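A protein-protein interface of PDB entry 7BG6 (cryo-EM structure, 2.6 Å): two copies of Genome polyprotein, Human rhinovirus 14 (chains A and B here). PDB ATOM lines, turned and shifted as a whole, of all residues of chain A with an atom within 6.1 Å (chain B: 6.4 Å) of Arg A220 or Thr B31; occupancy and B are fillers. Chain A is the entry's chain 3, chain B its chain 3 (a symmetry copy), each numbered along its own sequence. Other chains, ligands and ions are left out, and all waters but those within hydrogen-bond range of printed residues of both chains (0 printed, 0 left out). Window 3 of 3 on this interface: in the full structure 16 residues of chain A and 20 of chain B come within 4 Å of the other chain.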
ATOM      1  N   TYR A 103      27.810 -34.542 -18.617  1.00  0.00           N
ATOM      2  CA  TYR A 103      29.208 -34.376 -18.983  1.00  0.00           C
ATOM      3  C   TYR A 103      29.437 -32.967 -19.527  1.00  0.00           C
ATOM      4  O   TYR A 103      30.546 -32.633 -19.940  1.00  0.00           O
ATOM      5  CB  TYR A 103      29.652 -35.455 -19.975  1.00  0.00           C
ATOM      6  CG  TYR A 103      30.197 -36.708 -19.339  1.00  0.00           C
ATOM      7  CD1 TYR A 103      29.506 -37.909 -19.413  1.00  0.00           C
ATOM      8  CD2 TYR A 103      31.403 -36.694 -18.654  1.00  0.00           C
ATOM      9  CE1 TYR A 103      29.999 -39.063 -18.825  1.00  0.00           C
ATOM     10  CE2 TYR A 103      31.908 -37.838 -18.058  1.00  0.00           C
ATOM     11  CZ  TYR A 103      31.203 -39.027 -18.144  1.00  0.00           C
ATOM     12  OH  TYR A 103      31.700 -40.158 -17.563  1.00  0.00           O
ATOM     13  N   TYR A 104      28.374 -32.153 -19.519  1.00  0.00           N
ATOM     14  CA  TYR A 104      28.409 -30.801 -20.053  1.00  0.00           C
ATOM     15  C   TYR A 104      27.677 -29.854 -19.105  1.00  0.00           C
ATOM     16  O   TYR A 104      26.842 -30.284 -18.314  1.00  0.00           O
ATOM     17  CB  TYR A 104      27.843 -30.775 -21.476  1.00  0.00           C
ATOM     18  CG  TYR A 104      28.680 -31.521 -22.484  1.00  0.00           C
ATOM     19  CD1 TYR A 104      28.529 -32.888 -22.669  1.00  0.00           C
ATOM     20  CD2 TYR A 104      29.637 -30.866 -23.244  1.00  0.00           C
ATOM     21  CE1 TYR A 104      29.303 -33.585 -23.584  1.00  0.00           C
ATOM     22  CE2 TYR A 104      30.414 -31.547 -24.168  1.00  0.00           C
ATOM     23  CZ  TYR A 104      30.250 -32.911 -24.335  1.00  0.00           C
ATOM     24  OH  TYR A 104      31.013 -33.591 -25.239  1.00  0.00           O
ATOM     25  N   THR A 105      28.005 -28.561 -19.206  1.00  0.00           N
ATOM     26  CA  THR A 105      27.524 -27.558 -18.269  1.00  0.00           C
ATOM     27  C   THR A 105      26.319 -26.825 -18.854  1.00  0.00           C
ATOM     28  O   THR A 105      25.396 -26.468 -18.125  1.00  0.00           O
ATOM     29  CB  THR A 105      28.655 -26.599 -17.875  1.00  0.00           C
ATOM     30  OG1 THR A 105      29.749 -27.400 -17.429  1.00  0.00           O
ATOM     31  CG2 THR A 105      28.265 -25.623 -16.785  1.00  0.00           C
ATOM     32  N   HIS A 106      26.346 -26.603 -20.173  1.00  0.00           N
ATOM     33  CA  HIS A 106      25.285 -25.872 -20.845  1.00  0.00           C
ATOM     34  C   HIS A 106      24.579 -26.778 -21.848  1.00  0.00           C
ATOM     35  O   HIS A 106      25.212 -27.616 -22.488  1.00  0.00           O
ATOM     36  CB  HIS A 106      25.832 -24.607 -21.522  1.00  0.00           C
ATOM     37  CG  HIS A 106      26.701 -23.767 -20.647  1.00  0.00           C
ATOM     38  ND1 HIS A 106      27.847 -23.156 -21.118  1.00  0.00           N
ATOM     39  CD2 HIS A 106      26.607 -23.438 -19.339  1.00  0.00           C
ATOM     40  CE1 HIS A 106      28.416 -22.479 -20.141  1.00  0.00           C
ATOM     41  NE2 HIS A 106      27.676 -22.638 -19.039  1.00  0.00           N
ATOM     42  N   TRP A 107      23.261 -26.590 -21.969  1.00  0.00           N
ATOM     43  CA  TRP A 107      22.479 -27.264 -22.992  1.00  0.00           C
ATOM     44  C   TRP A 107      21.485 -26.292 -23.620  1.00  0.00           C
ATOM     45  O   TRP A 107      21.021 -25.355 -22.972  1.00  0.00           O
ATOM     46  CB  TRP A 107      21.794 -28.522 -22.440  1.00  0.00           C
ATOM     47  CG  TRP A 107      20.560 -28.263 -21.631  1.00  0.00           C
ATOM     48  CD1 TRP A 107      20.498 -27.961 -20.301  1.00  0.00           C
ATOM     49  CD2 TRP A 107      19.198 -28.302 -22.096  1.00  0.00           C
ATOM     50  NE1 TRP A 107      19.197 -27.803 -19.908  1.00  0.00           N
ATOM     51  CE2 TRP A 107      18.376 -28.007 -20.986  1.00  0.00           C
ATOM     52  CE3 TRP A 107      18.592 -28.553 -23.334  1.00  0.00           C
ATOM     53  CZ2 TRP A 107      16.985 -27.956 -21.082  1.00  0.00           C
ATOM     54  CZ3 TRP A 107      17.219 -28.505 -23.428  1.00  0.00           C
ATOM     55  CH2 TRP A 107      16.427 -28.209 -22.316  1.00  0.00           C
ATOM     56  N   GLN A 172      19.988 -18.145 -24.411  1.00  0.00           N
ATOM     57  CA  GLN A 172      20.234 -19.059 -25.517  1.00  0.00           C
ATOM     58  C   GLN A 172      20.635 -20.440 -25.003  1.00  0.00           C
ATOM     59  O   GLN A 172      20.480 -21.430 -25.716  1.00  0.00           O
ATOM     60  CB  GLN A 172      21.307 -18.502 -26.457  1.00  0.00           C
ATOM     61  CG  GLN A 172      20.887 -17.242 -27.202  1.00  0.00           C
ATOM     62  CD  GLN A 172      21.298 -15.970 -26.499  1.00  0.00           C
ATOM     63  OE1 GLN A 172      21.234 -15.857 -25.276  1.00  0.00           O
ATOM     64  NE2 GLN A 172      21.721 -14.988 -27.279  1.00  0.00           N
ATOM     65  N   PHE A 173      21.162 -20.492 -23.774  1.00  0.00           N
ATOM     66  CA  PHE A 173      21.622 -21.742 -23.191  1.00  0.00           C
ATOM     67  C   PHE A 173      21.119 -21.876 -21.757  1.00  0.00           C
ATOM     68  O   PHE A 173      21.084 -20.901 -21.009  1.00  0.00           O
ATOM     69  CB  PHE A 173      23.149 -21.839 -23.259  1.00  0.00           C
ATOM     70  CG  PHE A 173      23.696 -22.327 -24.577  1.00  0.00           C
ATOM     71  CD1 PHE A 173      24.033 -23.661 -24.754  1.00  0.00           C
ATOM     72  CD2 PHE A 173      23.874 -21.454 -25.641  1.00  0.00           C
ATOM     73  CE1 PHE A 173      24.535 -24.111 -25.967  1.00  0.00           C
ATOM     74  CE2 PHE A 173      24.375 -21.905 -26.853  1.00  0.00           C
ATOM     75  CZ  PHE A 173      24.706 -23.232 -27.013  1.00  0.00           C
ATOM     76  N   LYS A 218      22.149 -28.780 -28.419  1.00  0.00           N
ATOM     77  CA  LYS A 218      23.484 -28.240 -28.221  1.00  0.00           C
ATOM     78  C   LYS A 218      23.975 -28.584 -26.818  1.00  0.00           C
ATOM     79  O   LYS A 218      23.200 -28.571 -25.863  1.00  0.00           O
ATOM     80  CB  LYS A 218      23.481 -26.719 -28.410  1.00  0.00           C
ATOM     81  CG  LYS A 218      22.886 -26.214 -29.719  1.00  0.00           C
ATOM     82  CD  LYS A 218      22.834 -24.704 -29.809  1.00  0.00           C
ATOM     83  CE  LYS A 218      22.078 -24.206 -31.022  1.00  0.00           C
ATOM     84  NZ  LYS A 218      20.621 -24.455 -30.909  1.00  0.00           N
ATOM     85  N   LEU A 219      25.274 -28.894 -26.719  1.00  0.00           N
ATOM     86  CA  LEU A 219      25.959 -29.114 -25.455  1.00  0.00           C
ATOM     87  C   LEU A 219      27.360 -28.514 -25.546  1.00  0.00           C
ATOM     88  O   LEU A 219      28.007 -28.609 -26.587  1.00  0.00           O
ATOM     89  CB  LEU A 219      26.044 -30.619 -25.175  1.00  0.00           C
ATOM     90  CG  LEU A 219      24.755 -31.302 -24.716  1.00  0.00           C
ATOM     91  CD1 LEU A 219      24.900 -32.814 -24.778  1.00  0.00           C
ATOM     92  CD2 LEU A 219      24.372 -30.866 -23.310  1.00  0.00           C
ATOM     93  N   ARG A 220      27.819 -27.911 -24.444  1.00  0.00           N
ATOM     94  CA  ARG A 220      29.123 -27.269 -24.409  1.00  0.00           C
ATOM     95  C   ARG A 220      29.626 -27.172 -22.969  1.00  0.00           C
ATOM     96  O   ARG A 220      28.886 -27.451 -22.027  1.00  0.00           O
ATOM     97  CB  ARG A 220      29.064 -25.894 -25.084  1.00  0.00           C
ATOM     98  CG  ARG A 220      28.083 -24.928 -24.436  1.00  0.00           C
ATOM     99  CD  ARG A 220      28.076 -23.565 -25.095  1.00  0.00           C
ATOM    100  NE  ARG A 220      27.691 -22.547 -24.130  1.00  0.00           N
ATOM    101  CZ  ARG A 220      27.337 -21.305 -24.434  1.00  0.00           C
ATOM    102  NH1 ARG A 220      27.310 -20.908 -25.695  1.00  0.00           N
ATOM    103  NH2 ARG A 220      27.009 -20.460 -23.472  1.00  0.00           N
ATOM    104  N   LEU A 221      30.892 -26.752 -22.836  1.00  0.00           N
ATOM    105  CA  LEU A 221      31.620 -26.672 -21.579  1.00  0.00           C
ATOM    106  C   LEU A 221      31.571 -28.022 -20.866  1.00  0.00           C
ATOM    107  O   LEU A 221      30.734 -28.246 -19.994  1.00  0.00           O
ATOM    108  CB  LEU A 221      31.060 -25.536 -20.712  1.00  0.00           C
ATOM    109  CG  LEU A 221      32.025 -24.968 -19.671  1.00  0.00           C
ATOM    110  CD1 LEU A 221      31.727 -23.506 -19.385  1.00  0.00           C
ATOM    111  CD2 LEU A 221      32.001 -25.778 -18.388  1.00  0.00           C
ATOM    112  N   MET A 222      32.488 -28.913 -21.263  1.00  0.00           N
ATOM    113  CA  MET A 222      32.621 -30.235 -20.675  1.00  0.00           C
ATOM    114  C   MET A 222      32.894 -30.109 -19.179  1.00  0.00           C
ATOM    115  O   MET A 222      33.534 -29.155 -18.737  1.00  0.00           O
ATOM    116  CB  MET A 222      33.775 -31.007 -21.321  1.00  0.00           C
ATOM    117  CG  MET A 222      33.394 -31.706 -22.611  1.00  0.00           C
ATOM    118  SD  MET A 222      34.746 -32.701 -23.285  1.00  0.00           S
ATOM    119  CE  MET A 222      34.942 -33.926 -21.991  1.00  0.00           C
ATOM    120  N   TYR B  28      35.279 -25.278 -27.590  1.00  0.00           N
ATOM    121  CA  TYR B  28      34.101 -24.681 -26.985  1.00  0.00           C
ATOM    122  C   TYR B  28      33.551 -23.602 -27.915  1.00  0.00           C
ATOM    123  O   TYR B  28      34.302 -22.762 -28.409  1.00  0.00           O
ATOM    124  CB  TYR B  28      34.420 -24.125 -25.594  1.00  0.00           C
ATOM    125  CG  TYR B  28      33.322 -23.291 -24.977  1.00  0.00           C
ATOM    126  CD1 TYR B  28      32.400 -23.851 -24.107  1.00  0.00           C
ATOM    127  CD2 TYR B  28      33.201 -21.942 -25.268  1.00  0.00           C
ATOM    128  CE1 TYR B  28      31.387 -23.091 -23.540  1.00  0.00           C
ATOM    129  CE2 TYR B  28      32.196 -21.167 -24.710  1.00  0.00           C
ATOM    130  CZ  TYR B  28      31.286 -21.745 -23.844  1.00  0.00           C
ATOM    131  OH  TYR B  28      30.292 -20.990 -23.291  1.00  0.00           O
ATOM    132  N   GLU B  29      32.233 -23.643 -28.136  1.00  0.00           N
ATOM    133  CA  GLU B  29      31.539 -22.640 -28.926  1.00  0.00           C
ATOM    134  C   GLU B  29      30.958 -21.590 -27.982  1.00  0.00           C
ATOM    135  O   GLU B  29      30.125 -21.913 -27.137  1.00  0.00           O
ATOM    136  CB  GLU B  29      30.457 -23.302 -29.785  1.00  0.00           C
ATOM    137  CG  GLU B  29      29.716 -22.342 -30.701  1.00  0.00           C
ATOM    138  CD  GLU B  29      28.590 -21.540 -30.066  1.00  0.00           C
ATOM    139  OE1 GLU B  29      28.039 -21.988 -29.040  1.00  0.00           O
ATOM    140  OE2 GLU B  29      28.264 -20.465 -30.602  1.00  0.00           O
ATOM    141  N   PRO B  30      31.385 -20.309 -28.083  1.00  0.00           N
ATOM    142  CA  PRO B  30      30.785 -19.232 -27.294  1.00  0.00           C
ATOM    143  C   PRO B  30      29.431 -18.815 -27.862  1.00  0.00           C
ATOM    144  O   PRO B  30      29.222 -18.877 -29.071  1.00  0.00           O
ATOM    145  CB  PRO B  30      31.801 -18.088 -27.426  1.00  0.00           C
ATOM    146  CG  PRO B  30      32.465 -18.328 -28.768  1.00  0.00           C
ATOM    147  CD  PRO B  30      32.482 -19.834 -28.944  1.00  0.00           C
ATOM    148  N   THR B  31      28.532 -18.373 -26.973  1.00  0.00           N
ATOM    149  CA  THR B  31      27.172 -17.987 -27.327  1.00  0.00           C
ATOM    150  C   THR B  31      27.190 -17.043 -28.529  1.00  0.00           C
ATOM    151  O   THR B  31      28.054 -16.173 -28.618  1.00  0.00           O
ATOM    152  CB  THR B  31      26.451 -17.363 -26.124  1.00  0.00           C
ATOM    153  OG1 THR B  31      26.533 -18.279 -25.032  1.00  0.00           O
ATOM    154  CG2 THR B  31      24.999 -17.038 -26.398  1.00  0.00           C
ATOM    155  N   PRO B  32      26.242 -17.192 -29.488  1.00  0.00           N
ATOM    156  CA  PRO B  32      26.154 -16.291 -30.638  1.00  0.00           C
ATOM    157  C   PRO B  32      26.009 -14.828 -30.228  1.00  0.00           C
ATOM    158  O   PRO B  32      25.485 -14.527 -29.156  1.00  0.00           O
ATOM    159  CB  PRO B  32      24.864 -16.723 -31.351  1.00  0.00           C
ATOM    160  CG  PRO B  32      24.651 -18.157 -30.922  1.00  0.00           C
ATOM    161  CD  PRO B  32      25.220 -18.249 -29.523  1.00  0.00           C
ATOM    162  N   ARG B  33      26.482 -13.931 -31.099  1.00  0.00           N
ATOM    163  CA  ARG B  33      26.324 -12.500 -30.912  1.00  0.00           C
ATOM    164  C   ARG B  33      24.959 -12.076 -31.446  1.00  0.00           C
ATOM    165  O   ARG B  33      24.552 -12.499 -32.527  1.00  0.00           O
ATOM    166  CB  ARG B  33      27.435 -11.733 -31.637  1.00  0.00           C
ATOM    167  CG  ARG B  33      28.782 -11.763 -30.930  1.00  0.00           C
ATOM    168  CD  ARG B  33      29.844 -10.998 -31.697  1.00  0.00           C
ATOM    169  NE  ARG B  33      31.106 -10.931 -30.973  1.00  0.00           N
ATOM    170  CZ  ARG B  33      32.118 -11.782 -31.119  1.00  0.00           C
ATOM    171  NH1 ARG B  33      32.029 -12.787 -31.974  1.00  0.00           N
ATOM    172  NH2 ARG B  33      33.219 -11.621 -30.407  1.00  0.00           N
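No position is printed for both chains.
Of the 7 pairs that touch across the chains among the printed residues, none has its exchanged pair printed and touching as well.
Among the printed residues, merely in contact across the chains: His A106 with Tyr B28 (3.9 Å), Gln A172 with Thr B31 (3.9 Å), Arg A220 with Pro B30 (3.7 Å) and Leu A221 with Tyr B28 (3.5 Å).
Hydrophobic or aromatic side chains of chain A that line the printed part of chain B: His A106 and Leu A221.
Along chain A the printed residues that touch a printed residue of chain B span positions 106 to 221.
Of the 6 printed residues of chain B, 4 touch a printed residue of chain A.
Printed residues of chain B that touch a printed residue of chain A: Tyr B28, Glu B29, Pro B30 and Thr B31.
Hydrophobic or aromatic side chains of chain B that line the printed part of chain A: Tyr B28.
Among the printed residues, 7 pairs touch across the chains.
Among the printed residues, Asp or Glu carboxylates within 4 Å of a Lys or Arg side-chain nitrogen of the other chain: Arg A220 with Glu B29.
The backbone NH of Thr A105 lies within hydrogen-bond range of the backbone carbonyl oxygen of Arg A220 (3.2 Å).
O of Leu A221 lies within hydrogen-bond range of N of Thr A105.
The guanidinium group (NE) of Arg A220 is in hydrogen-bond range of a ring nitrogen (ND1) of His A106.
The guanidinium group (NE) of Arg A220 sits at hydrogen-bond distance from the side-chain hydroxyl (OH) of Tyr B28, 3.1 Å away.
The guanidinium group of Arg A220 lies within salt-bridge range of the side-chain carboxylate of Glu B29, 3.6 Å away.
The side-chain hydroxyl (OG1) of Thr B31 sits at hydrogen-bond distance from the guanidinium group (NH2) of Arg A220 (2.7 Å).
Of the printed residues of chain B, His A106 touches Tyr B28 (3.9 Å).
Arg A220 touches four residues of chain B.
Of the printed residues of chain B, Leu A221 touches Tyr B28.
Printed residues of chain A within 4 Å of Tyr B28: His A106, Arg A220 and Leu A221.
Printed residues of chain A within 4 Å of Glu B29: Arg A220.
Printed residues of chain A within 4 Å of Pro B30: Arg A220.
Thr B31 touches two residues of chain A.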
